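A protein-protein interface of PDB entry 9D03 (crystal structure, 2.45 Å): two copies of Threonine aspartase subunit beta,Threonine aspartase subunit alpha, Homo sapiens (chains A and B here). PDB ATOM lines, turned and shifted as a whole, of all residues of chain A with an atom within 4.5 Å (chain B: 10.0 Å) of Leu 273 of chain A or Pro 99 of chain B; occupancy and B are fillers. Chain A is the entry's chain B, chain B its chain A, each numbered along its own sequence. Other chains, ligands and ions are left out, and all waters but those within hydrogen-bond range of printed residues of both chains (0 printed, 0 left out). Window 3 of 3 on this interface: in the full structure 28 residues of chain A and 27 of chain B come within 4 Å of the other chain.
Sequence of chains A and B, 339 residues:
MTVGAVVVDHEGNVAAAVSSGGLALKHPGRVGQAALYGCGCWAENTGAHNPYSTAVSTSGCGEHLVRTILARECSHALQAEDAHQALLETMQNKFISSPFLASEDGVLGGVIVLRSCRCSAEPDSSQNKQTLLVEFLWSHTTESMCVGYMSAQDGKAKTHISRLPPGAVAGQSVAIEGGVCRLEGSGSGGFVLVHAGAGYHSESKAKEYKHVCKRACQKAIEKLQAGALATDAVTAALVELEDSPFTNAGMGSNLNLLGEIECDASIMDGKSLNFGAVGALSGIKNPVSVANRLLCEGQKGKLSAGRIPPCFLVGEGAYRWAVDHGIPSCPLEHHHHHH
O of Arg 67 of chain B lies within hydrogen-bond range of OH of Tyr 37 of chain A, 2.8 Å away.
The side-chain amide oxygen of Asn 274 of chain A sits at hydrogen-bond distance from the guanidinium group of Arg 67 of chain B (3.2 Å).
Of the 20 printed residues of chain B, 4 touch a printed residue of chain A.
Hydrophobic or aromatic side chains of chain B that line the printed part of chain A: Val 66 and Phe 100.
Printed residues of chain A that touch a printed residue of chain B: Tyr 37, Leu 273, Asn 274 and Phe 275.
Hydrophobic or aromatic side chains of chain A within 4 Å of the printed part of chain B: Tyr 37 and Leu 273.
Along chain A the printed residues that touch a printed residue of chain B span positions 37 to 275.
Among the printed residues, no Asp or Glu carboxylate lies within 4 Å of a Lys or Arg side-chain nitrogen of the other chain.
Tyr 37 of chain A touches Val 66 of chain B.
Tyr 37 of chain A touches Phe 100 of chain B.
NE of Arg 67 of chain B touches O of Leu 273 of chain A (3.8 Å).
CD1 of Leu 273 of chain A touches O of Pro 99 of chain B, 3.9 Å away.
CD1 of Phe 100 of chain B touches CD1 of Leu 273 of chain A, 3.5 Å away.
Phe 275 of chain A touches Arg 67 of chain B (N to NH1, 3.7 Å).
The side-chain hydroxyl of Ser 98 of chain B is in hydrogen-bond range of the backbone NH of Phe 100 of chain B, at 2.9 Å.
N of Asp 269 of chain A lies within hydrogen-bond range of O of Asn 274 of chain A, 2.9 Å away.
N of Asn 274 of chain A lies close to OG of Ser 272 of chain A (3.4 Å).
Leu 273 of chain A touches just these residues of chain B: Arg 67 (3.8 Å), Pro 99 (3.9 Å) and Phe 100 (3.5 Å).
Pro 99 of chain B touches just one residue of chain A: Leu 273.
No residue of chain B comes within 4 Å of Ser 272 of chain A.
Asn 274 of chain A touches one residue of chain B.
Of the printed residues of chain A, Val 66 of chain B touches Tyr 37.
Of the printed residues of chain A, Phe 100 of chain B touches Tyr 37 and Leu 273.
Leu 101 of chain B touches none of the printed residues of chain A.
The nearest residue of chain B that does not touch Leu 273 of chain A is Leu 101 of chain B (6.1 Å).
The nearest printed residue of chain A that does not touch Phe 100 of chain B is Met 268 of chain A (4.1 Å).
No position is printed for both chains.
Of the 8 pairs that touch across the chains among the printed residues, none has its exchanged pair printed and touching as well.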
ATOM      1  N   TYR A  37      23.043 -29.037  -9.195  1.00  0.00           N
ATOM      2  CA  TYR A  37      22.128 -27.950  -9.498  1.00  0.00           C
ATOM      3  C   TYR A  37      22.398 -27.380 -10.884  1.00  0.00           C
ATOM      4  O   TYR A  37      23.540 -27.105 -11.248  1.00  0.00           O
ATOM      5  CB  TYR A  37      22.264 -26.881  -8.408  1.00  0.00           C
ATOM      6  CG  TYR A  37      21.301 -25.708  -8.516  1.00  0.00           C
ATOM      7  CD1 TYR A  37      19.926 -25.887  -8.375  1.00  0.00           C
ATOM      8  CD2 TYR A  37      21.777 -24.423  -8.726  1.00  0.00           C
ATOM      9  CE1 TYR A  37      19.036 -24.825  -8.468  1.00  0.00           C
ATOM     10  CE2 TYR A  37      20.907 -23.345  -8.808  1.00  0.00           C
ATOM     11  CZ  TYR A  37      19.539 -23.548  -8.674  1.00  0.00           C
ATOM     12  OH  TYR A  37      18.682 -22.467  -8.746  1.00  0.00           O
ATOM     13  N   ALA A  43      13.811 -26.398 -13.802  1.00  0.00           N
ATOM     14  CA  ALA A  43      12.409 -26.040 -13.970  1.00  0.00           C
ATOM     15  C   ALA A  43      12.269 -24.577 -13.583  1.00  0.00           C
ATOM     16  O   ALA A  43      12.743 -24.154 -12.520  1.00  0.00           O
ATOM     17  CB  ALA A  43      11.483 -26.917 -13.121  1.00  0.00           C
ATOM     18  N   GLU A  44      11.638 -23.803 -14.447  1.00  0.00           N
ATOM     19  CA  GLU A  44      11.569 -22.370 -14.216  1.00  0.00           C
ATOM     20  C   GLU A  44      10.243 -21.877 -14.775  1.00  0.00           C
ATOM     21  O   GLU A  44      10.033 -21.948 -15.991  1.00  0.00           O
ATOM     22  CB  GLU A  44      12.753 -21.685 -14.884  1.00  0.00           C
ATOM     23  CG  GLU A  44      12.904 -20.251 -14.511  1.00  0.00           C
ATOM     24  CD  GLU A  44      14.249 -19.669 -14.903  1.00  0.00           C
ATOM     25  OE1 GLU A  44      14.437 -18.469 -14.621  1.00  0.00           O
ATOM     26  OE2 GLU A  44      15.099 -20.376 -15.499  1.00  0.00           O
ATOM     27  N   MET A 268      13.539 -30.031  -9.220  1.00  0.00           N
ATOM     28  CA  MET A 268      13.398 -28.586  -9.160  1.00  0.00           C
ATOM     29  C   MET A 268      11.952 -28.187  -9.407  1.00  0.00           C
ATOM     30  O   MET A 268      11.268 -28.797 -10.237  1.00  0.00           O
ATOM     31  CB  MET A 268      14.295 -27.896 -10.179  1.00  0.00           C
ATOM     32  CG  MET A 268      14.309 -26.403 -10.045  1.00  0.00           C
ATOM     33  SD  MET A 268      15.778 -25.813 -10.879  1.00  0.00           S
ATOM     34  CE  MET A 268      15.629 -24.032 -10.721  1.00  0.00           C
ATOM     35  N   ASP A 269      11.500 -27.166  -8.673  1.00  0.00           N
ATOM     36  CA  ASP A 269      10.144 -26.650  -8.775  1.00  0.00           C
ATOM     37  C   ASP A 269      10.146 -25.339  -9.555  1.00  0.00           C
ATOM     38  O   ASP A 269      10.819 -24.386  -9.166  1.00  0.00           O
ATOM     39  CB  ASP A 269       9.528 -26.439  -7.388  1.00  0.00           C
ATOM     40  CG  ASP A 269       8.103 -25.867  -7.466  1.00  0.00           C
ATOM     41  OD1 ASP A 269       7.263 -26.409  -8.215  1.00  0.00           O
ATOM     42  OD2 ASP A 269       7.820 -24.881  -6.778  1.00  0.00           O
ATOM     43  N   GLY A 270       9.372 -25.282 -10.639  1.00  0.00           N
ATOM     44  CA  GLY A 270       9.352 -24.084 -11.456  1.00  0.00           C
ATOM     45  C   GLY A 270       8.717 -22.887 -10.776  1.00  0.00           C
ATOM     46  O   GLY A 270       9.052 -21.740 -11.098  1.00  0.00           O
ATOM     47  N   LYS A 271       7.788 -23.123  -9.848  1.00  0.00           N
ATOM     48  CA  LYS A 271       7.092 -22.010  -9.206  1.00  0.00           C
ATOM     49  C   LYS A 271       7.972 -21.318  -8.172  1.00  0.00           C
ATOM     50  O   LYS A 271       8.127 -20.095  -8.194  1.00  0.00           O
ATOM     51  CB  LYS A 271       5.793 -22.495  -8.552  1.00  0.00           C
ATOM     52  CG  LYS A 271       4.912 -21.377  -8.016  1.00  0.00           C
ATOM     53  CD  LYS A 271       3.690 -21.947  -7.333  1.00  0.00           C
ATOM     54  CE  LYS A 271       2.638 -20.890  -7.052  1.00  0.00           C
ATOM     55  NZ  LYS A 271       2.626 -19.784  -8.049  1.00  0.00           N
ATOM     56  N   SER A 272       8.543 -22.078  -7.252  1.00  0.00           N
ATOM     57  CA  SER A 272       9.335 -21.528  -6.164  1.00  0.00           C
ATOM     58  C   SER A 272      10.820 -21.513  -6.455  1.00  0.00           C
ATOM     59  O   SER A 272      11.572 -20.895  -5.697  1.00  0.00           O
ATOM     60  CB  SER A 272       9.088 -22.337  -4.890  1.00  0.00           C
ATOM     61  OG  SER A 272       9.500 -23.675  -5.103  1.00  0.00           O
ATOM     62  N   LEU A 273      11.256 -22.193  -7.512  1.00  0.00           N
ATOM     63  CA  LEU A 273      12.663 -22.344  -7.880  1.00  0.00           C
ATOM     64  C   LEU A 273      13.458 -23.090  -6.814  1.00  0.00           C
ATOM     65  O   LEU A 273      14.695 -23.093  -6.844  1.00  0.00           O
ATOM     66  CB  LEU A 273      13.293 -20.992  -8.205  1.00  0.00           C
ATOM     67  CG  LEU A 273      12.525 -20.206  -9.282  1.00  0.00           C
ATOM     68  CD1 LEU A 273      13.035 -18.751  -9.367  1.00  0.00           C
ATOM     69  CD2 LEU A 273      12.576 -20.869 -10.672  1.00  0.00           C
ATOM     70  N   ASN A 274      12.771 -23.751  -5.893  1.00  0.00           N
ATOM     71  CA  ASN A 274      13.434 -24.607  -4.932  1.00  0.00           C
ATOM     72  C   ASN A 274      13.882 -25.904  -5.592  1.00  0.00           C
ATOM     73  O   ASN A 274      13.385 -26.316  -6.646  1.00  0.00           O
ATOM     74  CB  ASN A 274      12.520 -24.896  -3.753  1.00  0.00           C
ATOM     75  CG  ASN A 274      12.411 -23.706  -2.811  1.00  0.00           C
ATOM     76  OD1 ASN A 274      13.243 -22.789  -2.834  1.00  0.00           O
ATOM     77  ND2 ASN A 274      11.357 -23.696  -2.009  1.00  0.00           N
ATOM     78  N   PHE A 275      14.818 -26.553  -4.918  1.00  0.00           N
ATOM     79  CA  PHE A 275      15.641 -27.614  -5.460  1.00  0.00           C
ATOM     80  C   PHE A 275      15.959 -28.566  -4.321  1.00  0.00           C
ATOM     81  O   PHE A 275      16.152 -28.127  -3.188  1.00  0.00           O
ATOM     82  CB  PHE A 275      16.916 -27.013  -6.069  1.00  0.00           C
ATOM     83  CG  PHE A 275      17.937 -28.027  -6.519  1.00  0.00           C
ATOM     84  CD1 PHE A 275      17.818 -28.659  -7.750  1.00  0.00           C
ATOM     85  CD2 PHE A 275      19.065 -28.274  -5.759  1.00  0.00           C
ATOM     86  CE1 PHE A 275      18.767 -29.558  -8.195  1.00  0.00           C
ATOM     87  CE2 PHE A 275      20.026 -29.182  -6.198  1.00  0.00           C
ATOM     88  CZ  PHE A 275      19.886 -29.817  -7.421  1.00  0.00           C
ATOM     89  N   GLU B  63      22.330 -21.305   0.993  1.00  0.00           N
ATOM     90  CA  GLU B  63      22.128 -21.724  -0.383  1.00  0.00           C
ATOM     91  C   GLU B  63      22.094 -20.552  -1.359  1.00  0.00           C
ATOM     92  O   GLU B  63      21.751 -20.739  -2.527  1.00  0.00           O
ATOM     93  CB  GLU B  63      20.849 -22.557  -0.470  1.00  0.00           C
ATOM     94  CG  GLU B  63      20.866 -23.738   0.502  1.00  0.00           C
ATOM     95  CD  GLU B  63      22.079 -24.655   0.304  1.00  0.00           C
ATOM     96  OE1 GLU B  63      22.438 -24.934  -0.858  1.00  0.00           O
ATOM     97  OE2 GLU B  63      22.681 -25.095   1.307  1.00  0.00           O
ATOM     98  N   HIS B  64      22.508 -19.365  -0.919  1.00  0.00           N
ATOM     99  CA  HIS B  64      22.378 -18.169  -1.746  1.00  0.00           C
ATOM    100  C   HIS B  64      23.255 -18.228  -2.995  1.00  0.00           C
ATOM    101  O   HIS B  64      22.803 -17.871  -4.089  1.00  0.00           O
ATOM    102  CB  HIS B  64      22.713 -16.937  -0.907  1.00  0.00           C
ATOM    103  CG  HIS B  64      21.814 -16.753   0.276  1.00  0.00           C
ATOM    104  ND1 HIS B  64      22.153 -15.966   1.357  1.00  0.00           N
ATOM    105  CD2 HIS B  64      20.582 -17.248   0.544  1.00  0.00           C
ATOM    106  CE1 HIS B  64      21.169 -15.983   2.238  1.00  0.00           C
ATOM    107  NE2 HIS B  64      20.204 -16.755   1.768  1.00  0.00           N
ATOM    108  N   VAL B  66      24.562 -21.003  -4.419  1.00  0.00           N
ATOM    109  CA  VAL B  66      24.178 -22.137  -5.246  1.00  0.00           C
ATOM    110  C   VAL B  66      23.011 -21.742  -6.143  1.00  0.00           C
ATOM    111  O   VAL B  66      23.102 -21.800  -7.373  1.00  0.00           O
ATOM    112  CB  VAL B  66      23.809 -23.351  -4.368  1.00  0.00           C
ATOM    113  CG1 VAL B  66      23.235 -24.467  -5.223  1.00  0.00           C
ATOM    114  CG2 VAL B  66      24.995 -23.823  -3.536  1.00  0.00           C
ATOM    115  N   ARG B  67      21.913 -21.279  -5.524  1.00  0.00           N
ATOM    116  CA  ARG B  67      20.672 -20.974  -6.235  1.00  0.00           C
ATOM    117  C   ARG B  67      20.905 -20.047  -7.426  1.00  0.00           C
ATOM    118  O   ARG B  67      20.130 -20.078  -8.387  1.00  0.00           O
ATOM    119  CB  ARG B  67      19.629 -20.359  -5.281  1.00  0.00           C
ATOM    120  CG  ARG B  67      19.030 -21.293  -4.205  1.00  0.00           C
ATOM    121  CD  ARG B  67      18.132 -22.396  -4.793  1.00  0.00           C
ATOM    122  NE  ARG B  67      17.041 -22.822  -3.899  1.00  0.00           N
ATOM    123  CZ  ARG B  67      17.078 -23.895  -3.107  1.00  0.00           C
ATOM    124  NH1 ARG B  67      16.036 -24.215  -2.350  1.00  0.00           N
ATOM    125  NH2 ARG B  67      18.161 -24.659  -3.069  1.00  0.00           N
ATOM    126  N   THR B  68      21.974 -19.262  -7.409  1.00  0.00           N
ATOM    127  CA  THR B  68      22.189 -18.244  -8.418  1.00  0.00           C
ATOM    128  C   THR B  68      23.331 -18.572  -9.368  1.00  0.00           C
ATOM    129  O   THR B  68      23.572 -17.799 -10.303  1.00  0.00           O
ATOM    130  CB  THR B  68      22.417 -16.884  -7.750  1.00  0.00           C
ATOM    131  OG1 THR B  68      23.492 -16.985  -6.803  1.00  0.00           O
ATOM    132  CG2 THR B  68      21.159 -16.433  -7.043  1.00  0.00           C
ATOM    133  N   THR B  90      25.659  -7.433 -11.403  1.00  0.00           N
ATOM    134  CA  THR B  90      25.452  -8.835 -11.067  1.00  0.00           C
ATOM    135  C   THR B  90      25.140  -8.994  -9.592  1.00  0.00           C
ATOM    136  O   THR B  90      24.196  -9.701  -9.221  1.00  0.00           O
ATOM    137  CB  THR B  90      26.686  -9.669 -11.417  1.00  0.00           C
ATOM    138  OG1 THR B  90      27.022  -9.483 -12.796  1.00  0.00           O
ATOM    139  CG2 THR B  90      26.424 -11.171 -11.116  1.00  0.00           C
ATOM    140  N   GLN B  92      23.908  -6.880  -7.556  1.00  0.00           N
ATOM    141  CA  GLN B  92      22.618  -6.296  -7.221  1.00  0.00           C
ATOM    142  C   GLN B  92      21.456  -7.064  -7.842  1.00  0.00           C
ATOM    143  O   GLN B  92      20.468  -7.365  -7.163  1.00  0.00           O
ATOM    144  CB  GLN B  92      22.583  -4.834  -7.677  1.00  0.00           C
ATOM    145  CG  GLN B  92      23.424  -3.890  -6.837  1.00  0.00           C
ATOM    146  CD  GLN B  92      23.457  -2.462  -7.412  1.00  0.00           C
ATOM    147  OE1 GLN B  92      23.354  -2.257  -8.630  1.00  0.00           O
ATOM    148  NE2 GLN B  92      23.554  -1.472  -6.521  1.00  0.00           N
ATOM    149  N   ASN B  93      21.522  -7.309  -9.152  1.00  0.00           N
ATOM    150  CA  ASN B  93      20.408  -7.923  -9.868  1.00  0.00           C
ATOM    151  C   ASN B  93      20.411  -9.433  -9.739  1.00  0.00           C
ATOM    152  O   ASN B  93      19.407 -10.032  -9.347  1.00  0.00           O
ATOM    153  CB  ASN B  93      20.458  -7.535 -11.344  1.00  0.00           C
ATOM    154  CG  ASN B  93      20.420  -6.042 -11.548  1.00  0.00           C
ATOM    155  OD1 ASN B  93      19.710  -5.318 -10.846  1.00  0.00           O
ATOM    156  ND2 ASN B  93      21.218  -5.562 -12.492  1.00  0.00           N
ATOM    157  N   LYS B  94      21.539 -10.057 -10.061  1.00  0.00           N
ATOM    158  CA  LYS B  94      21.597 -11.508 -10.135  1.00  0.00           C
ATOM    159  C   LYS B  94      21.693 -12.156  -8.764  1.00  0.00           C
ATOM    160  O   LYS B  94      21.339 -13.328  -8.621  1.00  0.00           O
ATOM    161  CB  LYS B  94      22.789 -11.945 -10.993  1.00  0.00           C
ATOM    162  CG  LYS B  94      22.471 -12.231 -12.461  1.00  0.00           C
ATOM    163  CD  LYS B  94      22.201 -10.974 -13.242  1.00  0.00           C
ATOM    164  CE  LYS B  94      21.791 -11.303 -14.666  1.00  0.00           C
ATOM    165  NZ  LYS B  94      20.434 -11.909 -14.741  1.00  0.00           N
ATOM    166  N   PHE B  95      22.151 -11.422  -7.756  1.00  0.00           N
ATOM    167  CA  PHE B  95      22.403 -11.989  -6.442  1.00  0.00           C
ATOM    168  C   PHE B  95      21.427 -11.460  -5.402  1.00  0.00           C
ATOM    169  O   PHE B  95      20.655 -12.249  -4.854  1.00  0.00           O
ATOM    170  CB  PHE B  95      23.851 -11.714  -6.032  1.00  0.00           C
ATOM    171  CG  PHE B  95      24.252 -12.359  -4.744  1.00  0.00           C
ATOM    172  CD1 PHE B  95      24.169 -13.742  -4.583  1.00  0.00           C
ATOM    173  CD2 PHE B  95      24.735 -11.591  -3.694  1.00  0.00           C
ATOM    174  CE1 PHE B  95      24.560 -14.346  -3.391  1.00  0.00           C
ATOM    175  CE2 PHE B  95      25.116 -12.180  -2.501  1.00  0.00           C
ATOM    176  CZ  PHE B  95      25.041 -13.564  -2.352  1.00  0.00           C
ATOM    177  N   ILE B  96      21.357 -10.139  -5.190  1.00  0.00           N
ATOM    178  CA  ILE B  96      20.480  -9.623  -4.138  1.00  0.00           C
ATOM    179  C   ILE B  96      19.018  -9.743  -4.558  1.00  0.00           C
ATOM    180  O   ILE B  96      18.192 -10.292  -3.818  1.00  0.00           O
ATOM    181  CB  ILE B  96      20.841  -8.168  -3.796  1.00  0.00           C
ATOM    182  CG1 ILE B  96      21.965  -8.110  -2.769  1.00  0.00           C
ATOM    183  CG2 ILE B  96      19.591  -7.354  -3.308  1.00  0.00           C
ATOM    184  CD1 ILE B  96      22.328  -6.659  -2.410  1.00  0.00           C
ATOM    185  N   SER B  97      18.662  -9.210  -5.733  1.00  0.00           N
ATOM    186  CA  SER B  97      17.265  -9.203  -6.165  1.00  0.00           C
ATOM    187  C   SER B  97      16.952 -10.354  -7.125  1.00  0.00           C
ATOM    188  O   SER B  97      16.028 -10.255  -7.937  1.00  0.00           O
ATOM    189  CB  SER B  97      16.865  -7.844  -6.761  1.00  0.00           C
ATOM    190  OG  SER B  97      17.710  -7.450  -7.819  1.00  0.00           O
ATOM    191  N   SER B  98      17.706 -11.446  -7.037  1.00  0.00           N
ATOM    192  CA  SER B  98      17.439 -12.617  -7.859  1.00  0.00           C
ATOM    193  C   SER B  98      16.056 -13.181  -7.551  1.00  0.00           C
ATOM    194  O   SER B  98      15.620 -13.157  -6.394  1.00  0.00           O
ATOM    195  CB  SER B  98      18.490 -13.696  -7.605  1.00  0.00           C
ATOM    196  OG  SER B  98      18.001 -14.973  -7.985  1.00  0.00           O
ATOM    197  N   PRO B  99      15.341 -13.696  -8.554  1.00  0.00           N
ATOM    198  CA  PRO B  99      14.086 -14.399  -8.245  1.00  0.00           C
ATOM    199  C   PRO B  99      14.305 -15.660  -7.423  1.00  0.00           C
ATOM    200  O   PRO B  99      13.421 -16.041  -6.640  1.00  0.00           O
ATOM    201  CB  PRO B  99      13.514 -14.714  -9.633  1.00  0.00           C
ATOM    202  N   PHE B 100      15.473 -16.307  -7.577  1.00  0.00           N
ATOM    203  CA  PHE B 100      15.831 -17.500  -6.811  1.00  0.00           C
ATOM    204  C   PHE B 100      15.922 -17.236  -5.320  1.00  0.00           C
ATOM    205  O   PHE B 100      15.908 -18.187  -4.535  1.00  0.00           O
ATOM    206  CB  PHE B 100      17.175 -18.061  -7.287  1.00  0.00           C
ATOM    207  CG  PHE B 100      17.168 -18.507  -8.709  1.00  0.00           C
ATOM    208  CD1 PHE B 100      16.394 -19.591  -9.099  1.00  0.00           C
ATOM    209  CD2 PHE B 100      17.921 -17.845  -9.661  1.00  0.00           C
ATOM    210  CE1 PHE B 100      16.363 -20.012 -10.416  1.00  0.00           C
ATOM    211  CE2 PHE B 100      17.907 -18.264 -10.986  1.00  0.00           C
ATOM    212  CZ  PHE B 100      17.121 -19.349 -11.362  1.00  0.00           C
ATOM    213  N   LEU B 101      16.044 -15.973  -4.913  1.00  0.00           N
ATOM    214  CA  LEU B 101      16.192 -15.611  -3.509  1.00  0.00           C
ATOM    215  C   LEU B 101      15.139 -14.589  -3.101  1.00  0.00           C
ATOM    216  O   LEU B 101      15.372 -13.770  -2.210  1.00  0.00           O
ATOM    217  CB  LEU B 101      17.597 -15.074  -3.232  1.00  0.00           C
ATOM    218  CG  LEU B 101      18.765 -15.910  -3.755  1.00  0.00           C
ATOM    219  CD1 LEU B 101      20.058 -15.172  -3.579  1.00  0.00           C
ATOM    220  CD2 LEU B 101      18.825 -17.266  -3.054  1.00  0.00           C
ATOM    221  N   ALA B 102      13.977 -14.617  -3.752  1.00  0.00           N
ATOM    222  CA  ALA B 102      12.962 -13.610  -3.468  1.00  0.00           C
ATOM    223  C   ALA B 102      12.342 -13.800  -2.087  1.00  0.00           C
ATOM    224  O   ALA B 102      11.875 -12.826  -1.485  1.00  0.00           O
ATOM    225  CB  ALA B 102      11.885 -13.637  -4.551  1.00  0.00           C
ATOM    226  N   SER B 103      12.340 -15.028  -1.563  1.00  0.00           N
ATOM    227  CA  SER B 103      11.715 -15.341  -0.280  1.00  0.00           C
ATOM    228  C   SER B 103      12.635 -15.102   0.915  1.00  0.00           C
ATOM    229  O   SER B 103      12.280 -15.478   2.040  1.00  0.00           O
ATOM    230  CB  SER B 103      11.231 -16.795  -0.270  1.00  0.00           C
ATOM    231  OG  SER B 103      10.196 -16.996  -1.217  1.00  0.00           O
ATOM    232  N   GLU B 104      13.791 -14.472   0.701  1.00  0.00           N
ATOM    233  CA  GLU B 104      14.809 -14.294   1.727  1.00  0.00           C
ATOM    234  C   GLU B 104      14.787 -12.876   2.291  1.00  0.00           C
ATOM    235  O   GLU B 104      14.707 -11.896   1.541  1.00  0.00           O
ATOM    236  CB  GLU B 104      16.199 -14.589   1.156  1.00  0.00           C
ATOM    237  CG  GLU B 104      16.459 -16.049   0.878  1.00  0.00           C
ATOM    238  CD  GLU B 104      16.510 -16.868   2.150  1.00  0.00           C
ATOM    239  OE1 GLU B 104      16.949 -16.324   3.188  1.00  0.00           O
ATOM    240  OE2 GLU B 104      16.102 -18.049   2.116  1.00  0.00           O
ATOM    241  N   VAL B 107      20.495 -11.346   1.805  1.00  0.00           N
ATOM    242  CA  VAL B 107      21.324 -12.247   0.997  1.00  0.00           C
ATOM    243  C   VAL B 107      22.790 -11.920   1.265  1.00  0.00           C
ATOM    244  O   VAL B 107      23.277 -10.860   0.851  1.00  0.00           O
ATOM    245  CB  VAL B 107      21.006 -12.108  -0.505  1.00  0.00           C
ATOM    246  CG1 VAL B 107      21.939 -12.933  -1.318  1.00  0.00           C
ATOM    247  CG2 VAL B 107      19.543 -12.509  -0.802  1.00  0.00           C
